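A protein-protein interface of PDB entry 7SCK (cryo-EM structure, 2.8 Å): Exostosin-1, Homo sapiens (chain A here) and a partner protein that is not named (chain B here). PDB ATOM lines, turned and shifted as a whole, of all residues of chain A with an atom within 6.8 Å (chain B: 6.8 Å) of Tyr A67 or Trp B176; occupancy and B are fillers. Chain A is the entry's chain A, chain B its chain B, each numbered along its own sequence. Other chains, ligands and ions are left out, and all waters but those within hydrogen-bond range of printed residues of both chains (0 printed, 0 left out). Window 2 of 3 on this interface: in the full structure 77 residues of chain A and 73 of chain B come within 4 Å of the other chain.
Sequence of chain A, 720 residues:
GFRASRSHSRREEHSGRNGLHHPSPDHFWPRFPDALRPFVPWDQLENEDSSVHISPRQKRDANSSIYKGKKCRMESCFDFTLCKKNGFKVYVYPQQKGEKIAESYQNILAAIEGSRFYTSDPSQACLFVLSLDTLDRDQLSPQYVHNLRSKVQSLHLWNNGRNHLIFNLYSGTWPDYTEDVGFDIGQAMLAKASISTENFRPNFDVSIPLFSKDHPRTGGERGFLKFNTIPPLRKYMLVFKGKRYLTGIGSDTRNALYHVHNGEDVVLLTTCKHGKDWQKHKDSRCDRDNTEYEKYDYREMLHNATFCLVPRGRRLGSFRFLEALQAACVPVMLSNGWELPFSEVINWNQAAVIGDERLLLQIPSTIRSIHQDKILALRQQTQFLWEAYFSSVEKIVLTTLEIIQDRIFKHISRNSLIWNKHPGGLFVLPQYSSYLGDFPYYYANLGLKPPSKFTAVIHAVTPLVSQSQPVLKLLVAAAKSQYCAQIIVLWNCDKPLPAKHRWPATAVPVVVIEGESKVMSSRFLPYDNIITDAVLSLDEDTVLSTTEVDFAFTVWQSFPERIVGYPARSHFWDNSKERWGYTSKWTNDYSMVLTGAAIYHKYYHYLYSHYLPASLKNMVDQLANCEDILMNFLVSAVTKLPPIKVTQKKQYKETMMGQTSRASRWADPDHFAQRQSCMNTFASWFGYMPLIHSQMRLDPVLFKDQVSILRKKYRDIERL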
ATOM      1  N   SER A  64      38.257 -21.199   2.996  1.00  0.00           N
ATOM      2  CA  SER A  64      38.028 -19.781   2.744  1.00  0.00           C
ATOM      3  C   SER A  64      37.888 -19.495   1.252  1.00  0.00           C
ATOM      4  O   SER A  64      37.283 -18.501   0.856  1.00  0.00           O
ATOM      5  CB  SER A  64      39.164 -18.941   3.331  1.00  0.00           C
ATOM      6  OG  SER A  64      38.974 -17.566   3.048  1.00  0.00           O
ATOM      7  N   SER A  65      38.463 -20.371   0.427  1.00  0.00           N
ATOM      8  CA  SER A  65      38.362 -20.206  -1.018  1.00  0.00           C
ATOM      9  C   SER A  65      36.984 -20.602  -1.533  1.00  0.00           C
ATOM     10  O   SER A  65      36.491 -20.022  -2.507  1.00  0.00           O
ATOM     11  CB  SER A  65      39.448 -21.023  -1.717  1.00  0.00           C
ATOM     12  OG  SER A  65      39.385 -20.859  -3.123  1.00  0.00           O
ATOM     13  N   ILE A  66      36.352 -21.591  -0.900  1.00  0.00           N
ATOM     14  CA  ILE A  66      35.041 -22.045  -1.348  1.00  0.00           C
ATOM     15  C   ILE A  66      33.971 -21.004  -1.039  1.00  0.00           C
ATOM     16  O   ILE A  66      33.080 -20.748  -1.857  1.00  0.00           O
ATOM     17  CB  ILE A  66      34.707 -23.407  -0.715  1.00  0.00           C
ATOM     18  CG1 ILE A  66      35.794 -24.429  -1.051  1.00  0.00           C
ATOM     19  CG2 ILE A  66      33.347 -23.898  -1.187  1.00  0.00           C
ATOM     20  CD1 ILE A  66      35.545 -25.802  -0.467  1.00  0.00           C
ATOM     21  N   TYR A  67      34.038 -20.386   0.139  1.00  0.00           N
ATOM     22  CA  TYR A  67      32.980 -19.516   0.637  1.00  0.00           C
ATOM     23  C   TYR A  67      33.404 -18.050   0.692  1.00  0.00           C
ATOM     24  O   TYR A  67      33.069 -17.332   1.633  1.00  0.00           O
ATOM     25  CB  TYR A  67      32.521 -19.969   2.018  1.00  0.00           C
ATOM     26  CG  TYR A  67      32.223 -21.446   2.136  1.00  0.00           C
ATOM     27  CD1 TYR A  67      31.014 -21.968   1.700  1.00  0.00           C
ATOM     28  CD2 TYR A  67      33.144 -22.314   2.704  1.00  0.00           C
ATOM     29  CE1 TYR A  67      30.736 -23.317   1.814  1.00  0.00           C
ATOM     30  CE2 TYR A  67      32.874 -23.665   2.825  1.00  0.00           C
ATOM     31  CZ  TYR A  67      31.670 -24.161   2.379  1.00  0.00           C
ATOM     32  OH  TYR A  67      31.398 -25.502   2.497  1.00  0.00           O
ATOM     33  N   LYS A  68      34.151 -17.584  -0.304  1.00  0.00           N
ATOM     34  CA  LYS A  68      34.546 -16.174  -0.356  1.00  0.00           C
ATOM     35  C   LYS A  68      33.620 -15.356  -1.252  1.00  0.00           C
ATOM     36  O   LYS A  68      34.065 -14.642  -2.148  1.00  0.00           O
ATOM     37  CB  LYS A  68      35.995 -16.051  -0.814  1.00  0.00           C
ATOM     38  CG  LYS A  68      36.327 -16.825  -2.082  1.00  0.00           C
ATOM     39  CD  LYS A  68      37.413 -16.128  -2.888  1.00  0.00           C
ATOM     40  CE  LYS A  68      38.644 -15.841  -2.042  1.00  0.00           C
ATOM     41  NZ  LYS A  68      39.313 -17.085  -1.576  1.00  0.00           N
ATOM     42  N   GLY A  69      32.315 -15.441  -1.008  1.00  0.00           N
ATOM     43  CA  GLY A  69      31.367 -14.741  -1.850  1.00  0.00           C
ATOM     44  C   GLY A  69      30.137 -14.244  -1.124  1.00  0.00           C
ATOM     45  O   GLY A  69      30.239 -13.543  -0.115  1.00  0.00           O
ATOM     46  N   LYS A  70      28.959 -14.586  -1.650  1.00  0.00           N
ATOM     47  CA  LYS A  70      27.712 -14.272  -0.966  1.00  0.00           C
ATOM     48  C   LYS A  70      27.612 -14.982   0.376  1.00  0.00           C
ATOM     49  O   LYS A  70      26.859 -14.538   1.250  1.00  0.00           O
ATOM     50  CB  LYS A  70      26.524 -14.646  -1.853  1.00  0.00           C
ATOM     51  CG  LYS A  70      25.175 -14.174  -1.342  1.00  0.00           C
ATOM     52  CD  LYS A  70      24.052 -14.577  -2.284  1.00  0.00           C
ATOM     53  CE  LYS A  70      23.967 -16.088  -2.432  1.00  0.00           C
ATOM     54  NZ  LYS A  70      22.856 -16.496  -3.335  1.00  0.00           N
ATOM     55  N   LYS A  71      28.365 -16.067   0.564  1.00  0.00           N
ATOM     56  CA  LYS A  71      28.398 -16.805   1.819  1.00  0.00           C
ATOM     57  C   LYS A  71      29.513 -16.338   2.744  1.00  0.00           C
ATOM     58  O   LYS A  71      30.023 -17.130   3.545  1.00  0.00           O
ATOM     59  CB  LYS A  71      28.536 -18.300   1.535  1.00  0.00           C
ATOM     60  CG  LYS A  71      27.538 -18.829   0.529  1.00  0.00           C
ATOM     61  CD  LYS A  71      27.717 -20.318   0.314  1.00  0.00           C
ATOM     62  CE  LYS A  71      27.555 -21.084   1.616  1.00  0.00           C
ATOM     63  NZ  LYS A  71      26.232 -20.825   2.249  1.00  0.00           N
ATOM     64  N   CYS A  72      29.911 -15.077   2.649  1.00  0.00           N
ATOM     65  CA  CYS A  72      31.031 -14.583   3.434  1.00  0.00           C
ATOM     66  C   CYS A  72      30.695 -14.559   4.918  1.00  0.00           C
ATOM     67  O   CYS A  72      29.568 -14.254   5.316  1.00  0.00           O
ATOM     68  CB  CYS A  72      31.428 -13.185   2.968  1.00  0.00           C
ATOM     69  SG  CYS A  72      32.761 -13.145   1.751  1.00  0.00           S
ATOM     70  N   ARG A  73      31.688 -14.884   5.738  1.00  0.00           N
ATOM     71  CA  ARG A  73      31.573 -14.862   7.186  1.00  0.00           C
ATOM     72  C   ARG A  73      32.767 -14.115   7.762  1.00  0.00           C
ATOM     73  O   ARG A  73      33.746 -13.833   7.067  1.00  0.00           O
ATOM     74  CB  ARG A  73      31.497 -16.281   7.761  1.00  0.00           C
ATOM     75  CG  ARG A  73      30.287 -17.069   7.312  1.00  0.00           C
ATOM     76  CD  ARG A  73      29.007 -16.385   7.736  1.00  0.00           C
ATOM     77  NE  ARG A  73      27.825 -17.167   7.392  1.00  0.00           N
ATOM     78  CZ  ARG A  73      27.150 -17.048   6.256  1.00  0.00           C
ATOM     79  NH1 ARG A  73      27.523 -16.195   5.317  1.00  0.00           N
ATOM     80  NH2 ARG A  73      26.074 -17.803   6.059  1.00  0.00           N
ATOM     81  N   GLU A  75      34.925 -15.210   9.828  1.00  0.00           N
ATOM     82  CA  GLU A  75      36.121 -16.031   9.953  1.00  0.00           C
ATOM     83  C   GLU A  75      36.769 -16.355   8.614  1.00  0.00           C
ATOM     84  O   GLU A  75      37.867 -16.918   8.601  1.00  0.00           O
ATOM     85  CB  GLU A  75      35.806 -17.332  10.691  1.00  0.00           C
ATOM     86  CG  GLU A  75      34.961 -18.308   9.908  1.00  0.00           C
ATOM     87  CD  GLU A  75      33.483 -18.019  10.024  1.00  0.00           C
ATOM     88  OE1 GLU A  75      33.117 -17.051  10.724  1.00  0.00           O
ATOM     89  OE2 GLU A  75      32.687 -18.765   9.420  1.00  0.00           O
ATOM     90  N   SER A  76      36.125 -16.022   7.497  1.00  0.00           N
ATOM     91  CA  SER A  76      36.704 -16.213   6.176  1.00  0.00           C
ATOM     92  C   SER A  76      36.975 -14.900   5.460  1.00  0.00           C
ATOM     93  O   SER A  76      38.108 -14.648   5.039  1.00  0.00           O
ATOM     94  CB  SER A  76      35.788 -17.096   5.316  1.00  0.00           C
ATOM     95  OG  SER A  76      34.548 -16.460   5.071  1.00  0.00           O
ATOM     96  N   CYS A  77      35.967 -14.048   5.315  1.00  0.00           N
ATOM     97  CA  CYS A  77      36.137 -12.772   4.625  1.00  0.00           C
ATOM     98  C   CYS A  77      36.432 -11.640   5.601  1.00  0.00           C
ATOM     99  O   CYS A  77      35.811 -10.582   5.566  1.00  0.00           O
ATOM    100  CB  CYS A  77      34.900 -12.471   3.792  1.00  0.00           C
ATOM    101  SG  CYS A  77      34.361 -13.864   2.773  1.00  0.00           S
ATOM    102  N   GLN A 187      34.263  -8.473  -0.507  1.00  0.00           N
ATOM    103  CA  GLN A 187      34.277  -9.128   0.793  1.00  0.00           C
ATOM    104  C   GLN A 187      33.837  -8.212   1.926  1.00  0.00           C
ATOM    105  O   GLN A 187      33.817  -8.645   3.080  1.00  0.00           O
ATOM    106  CB  GLN A 187      35.674  -9.680   1.093  1.00  0.00           C
ATOM    107  CG  GLN A 187      36.032 -10.917   0.291  1.00  0.00           C
ATOM    108  CD  GLN A 187      37.390 -11.474   0.661  1.00  0.00           C
ATOM    109  OE1 GLN A 187      38.205 -10.791   1.281  1.00  0.00           O
ATOM    110  NE2 GLN A 187      37.639 -12.724   0.288  1.00  0.00           N
ATOM    111  N   LEU B  39      19.454 -23.815   1.194  1.00  0.00           N
ATOM    112  CA  LEU B  39      19.855 -22.872   2.233  1.00  0.00           C
ATOM    113  C   LEU B  39      18.954 -21.645   2.270  1.00  0.00           C
ATOM    114  O   LEU B  39      18.746 -21.065   3.341  1.00  0.00           O
ATOM    115  CB  LEU B  39      21.310 -22.457   2.032  1.00  0.00           C
ATOM    116  CG  LEU B  39      22.335 -23.583   2.177  1.00  0.00           C
ATOM    117  CD1 LEU B  39      23.742 -23.066   1.923  1.00  0.00           C
ATOM    118  CD2 LEU B  39      22.233 -24.222   3.553  1.00  0.00           C
ATOM    119  N   ASN B 156      30.163 -32.642   5.692  1.00  0.00           N
ATOM    120  CA  ASN B 156      29.565 -31.390   5.246  1.00  0.00           C
ATOM    121  C   ASN B 156      28.966 -30.569   6.381  1.00  0.00           C
ATOM    122  O   ASN B 156      28.437 -29.482   6.122  1.00  0.00           O
ATOM    123  CB  ASN B 156      28.485 -31.669   4.196  1.00  0.00           C
ATOM    124  CG  ASN B 156      29.034 -32.368   2.966  1.00  0.00           C
ATOM    125  OD1 ASN B 156      30.189 -32.170   2.591  1.00  0.00           O
ATOM    126  ND2 ASN B 156      28.205 -33.191   2.333  1.00  0.00           N
ATOM    127  N   THR B 157      29.038 -31.059   7.622  1.00  0.00           N
ATOM    128  CA  THR B 157      28.476 -30.370   8.789  1.00  0.00           C
ATOM    129  C   THR B 157      26.985 -30.097   8.608  1.00  0.00           C
ATOM    130  O   THR B 157      26.466 -29.061   9.028  1.00  0.00           O
ATOM    131  CB  THR B 157      29.234 -29.075   9.098  1.00  0.00           C
ATOM    132  OG1 THR B 157      28.992 -28.112   8.064  1.00  0.00           O
ATOM    133  CG2 THR B 157      30.730 -29.342   9.196  1.00  0.00           C
ATOM    134  N   PHE B 173      26.498 -28.235  13.137  1.00  0.00           N
ATOM    135  CA  PHE B 173      26.121 -27.129  12.273  1.00  0.00           C
ATOM    136  C   PHE B 173      27.272 -26.143  12.187  1.00  0.00           C
ATOM    137  O   PHE B 173      27.796 -25.705  13.216  1.00  0.00           O
ATOM    138  CB  PHE B 173      24.875 -26.411  12.799  1.00  0.00           C
ATOM    139  CG  PHE B 173      23.583 -26.953  12.269  1.00  0.00           C
ATOM    140  CD1 PHE B 173      23.558 -27.773  11.159  1.00  0.00           C
ATOM    141  CD2 PHE B 173      22.389 -26.630  12.881  1.00  0.00           C
ATOM    142  CE1 PHE B 173      22.368 -28.262  10.676  1.00  0.00           C
ATOM    143  CE2 PHE B 173      21.201 -27.120  12.402  1.00  0.00           C
ATOM    144  CZ  PHE B 173      21.189 -27.934  11.299  1.00  0.00           C
ATOM    145  N   SER B 174      27.660 -25.796  10.969  1.00  0.00           N
ATOM    146  CA  SER B 174      28.554 -24.676  10.737  1.00  0.00           C
ATOM    147  C   SER B 174      27.726 -23.453  10.379  1.00  0.00           C
ATOM    148  O   SER B 174      26.538 -23.548  10.071  1.00  0.00           O
ATOM    149  CB  SER B 174      29.556 -24.998   9.628  1.00  0.00           C
ATOM    150  OG  SER B 174      28.890 -25.269   8.407  1.00  0.00           O
ATOM    151  N   THR B 175      28.367 -22.288  10.419  1.00  0.00           N
ATOM    152  CA  THR B 175      27.649 -21.059  10.112  1.00  0.00           C
ATOM    153  C   THR B 175      27.257 -20.960   8.645  1.00  0.00           C
ATOM    154  O   THR B 175      26.488 -20.063   8.288  1.00  0.00           O
ATOM    155  CB  THR B 175      28.487 -19.850  10.511  1.00  0.00           C
ATOM    156  OG1 THR B 175      27.709 -18.658  10.358  1.00  0.00           O
ATOM    157  CG2 THR B 175      29.712 -19.760   9.638  1.00  0.00           C
ATOM    158  N   TRP B 176      27.767 -21.846   7.794  1.00  0.00           N
ATOM    159  CA  TRP B 176      27.377 -21.885   6.393  1.00  0.00           C
ATOM    160  C   TRP B 176      26.210 -22.821   6.135  1.00  0.00           C
ATOM    161  O   TRP B 176      25.376 -22.532   5.271  1.00  0.00           O
ATOM    162  CB  TRP B 176      28.564 -22.308   5.523  1.00  0.00           C
ATOM    163  CG  TRP B 176      29.700 -21.350   5.570  1.00  0.00           C
ATOM    164  CD1 TRP B 176      29.780 -20.152   4.935  1.00  0.00           C
ATOM    165  CD2 TRP B 176      30.922 -21.504   6.294  1.00  0.00           C
ATOM    166  NE1 TRP B 176      30.975 -19.545   5.217  1.00  0.00           N
ATOM    167  CE2 TRP B 176      31.696 -20.356   6.052  1.00  0.00           C
ATOM    168  CE3 TRP B 176      31.438 -22.501   7.125  1.00  0.00           C
ATOM    169  CZ2 TRP B 176      32.957 -20.177   6.605  1.00  0.00           C
ATOM    170  CZ3 TRP B 176      32.690 -22.322   7.674  1.00  0.00           C
ATOM    171  CH2 TRP B 176      33.436 -21.169   7.413  1.00  0.00           C
ATOM    172  N   THR B 177      26.127 -23.932   6.858  1.00  0.00           N
ATOM    173  CA  THR B 177      25.040 -24.882   6.691  1.00  0.00           C
ATOM    174  C   THR B 177      23.887 -24.619   7.646  1.00  0.00           C
ATOM    175  O   THR B 177      23.029 -25.490   7.818  1.00  0.00           O
ATOM    176  CB  THR B 177      25.551 -26.312   6.880  1.00  0.00           C
ATOM    177  OG1 THR B 177      25.939 -26.507   8.242  1.00  0.00           O
ATOM    178  CG2 THR B 177      26.748 -26.569   5.987  1.00  0.00           C
ATOM    179  N   TYR B 178      23.846 -23.446   8.268  1.00  0.00           N
ATOM    180  CA  TYR B 178      22.860 -23.118   9.286  1.00  0.00           C
ATOM    181  C   TYR B 178      21.916 -22.043   8.769  1.00  0.00           C
ATOM    182  O   TYR B 178      22.363 -20.977   8.336  1.00  0.00           O
ATOM    183  CB  TYR B 178      23.554 -22.639  10.559  1.00  0.00           C
ATOM    184  CG  TYR B 178      22.628 -22.273  11.688  1.00  0.00           C
ATOM    185  CD1 TYR B 178      21.773 -23.213  12.242  1.00  0.00           C
ATOM    186  CD2 TYR B 178      22.629 -20.996  12.221  1.00  0.00           C
ATOM    187  CE1 TYR B 178      20.934 -22.884  13.282  1.00  0.00           C
ATOM    188  CE2 TYR B 178      21.796 -20.658  13.260  1.00  0.00           C
ATOM    189  CZ  TYR B 178      20.950 -21.606  13.787  1.00  0.00           C
ATOM    190  OH  TYR B 178      20.113 -21.272  14.825  1.00  0.00           O
ATOM    191  N   ARG B 179      20.617 -22.322   8.826  1.00  0.00           N
ATOM    192  CA  ARG B 179      19.599 -21.311   8.583  1.00  0.00           C
ATOM    193  C   ARG B 179      19.227 -20.680   9.916  1.00  0.00           C
ATOM    194  O   ARG B 179      18.907 -21.391  10.872  1.00  0.00           O
ATOM    195  CB  ARG B 179      18.370 -21.927   7.926  1.00  0.00           C
ATOM    196  CG  ARG B 179      18.685 -22.860   6.784  1.00  0.00           C
ATOM    197  CD  ARG B 179      17.560 -23.843   6.590  1.00  0.00           C
ATOM    198  NE  ARG B 179      17.880 -24.844   5.584  1.00  0.00           N
ATOM    199  CZ  ARG B 179      17.171 -25.943   5.373  1.00  0.00           C
ATOM    200  NH1 ARG B 179      16.107 -26.229   6.100  1.00  0.00           N
ATOM    201  NH2 ARG B 179      17.542 -26.777   4.406  1.00  0.00           N
ATOM    202  N   ASP B 302      36.646 -23.869  14.795  1.00  0.00           N
ATOM    203  CA  ASP B 302      36.695 -22.533  14.208  1.00  0.00           C
ATOM    204  C   ASP B 302      35.299 -22.013  13.883  1.00  0.00           C
ATOM    205  O   ASP B 302      34.924 -20.911  14.300  1.00  0.00           O
ATOM    206  CB  ASP B 302      37.570 -22.548  12.953  1.00  0.00           C
ATOM    207  CG  ASP B 302      37.680 -21.183  12.301  1.00  0.00           C
ATOM    208  OD1 ASP B 302      38.328 -20.291  12.888  1.00  0.00           O
ATOM    209  OD2 ASP B 302      37.123 -21.003  11.198  1.00  0.00           O
ATOM    210  N   SER B 303      34.512 -22.795  13.151  1.00  0.00           N
ATOM    211  CA  SER B 303      33.192 -22.378  12.682  1.00  0.00           C
ATOM    212  C   SER B 303      32.176 -23.411  13.147  1.00  0.00           C
ATOM    213  O   SER B 303      31.863 -24.357  12.423  1.00  0.00           O
ATOM    214  CB  SER B 303      33.174 -22.226  11.166  1.00  0.00           C
ATOM    215  OG  SER B 303      34.178 -21.326  10.731  1.00  0.00           O
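Hydrophobic or aromatic side chains of chain B that line the printed part of chain A: Leu B39 and Trp B176.
Tyr A67 touches one residue of chain B. Printed residues of chain A within 4 Å of Asp B302: Glu A75. Of the printed residues of chain A, Ser B303 touches Glu A75 (3.2 Å). Printed residues of chain B within 4 Å of Glu A75: Thr B175 (3.1 Å), Trp B176 (3.2 Å), Asp B302 (3.7 Å) and Ser B303 (3.2 Å). Printed residues of chain A within 4 Å of Leu B39: Lys A71 (3.4 Å). The nearest residue of chain A that does not touch Trp B176 is Ser A76 (4.3 Å).
NE1 of Trp B176 lies within hydrogen-bond range of O of Lys A71. O of Thr B175 is in hydrogen-bond range of NH2 of Arg A73 (3.2 Å). OG of Ser B303 sits close to OE2 of Glu A75, 3.2 Å away.
Tyr A67 touches Trp B176. Leu B39 touches Lys A71 (CD1 to NZ, 3.4 Å). CG of Arg A73 touches NE1 of Trp B176, 3.3 Å away. Thr B175 touches Glu A75 (CG2 to OE2, 3.1 Å). OE2 of Glu A75 touches CZ2 of Trp B176, 3.2 Å away. CG of Glu A75 touches OD2 of Asp B302, at 3.7 Å.
NH1 of Arg A73 lies within hydrogen-bond range of O of Lys A71 (3.2 Å). N of Arg A73 sits at hydrogen-bond distance from OG of Ser A76, 3.3 Å away. OD2 of Asp B302 is in hydrogen-bond range of OG of Ser B303 (3.0 Å). The side-chain sulfur of Cys A77 is disulfide-bonded to the side-chain sulfur of Cys A72 (2.0 Å).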
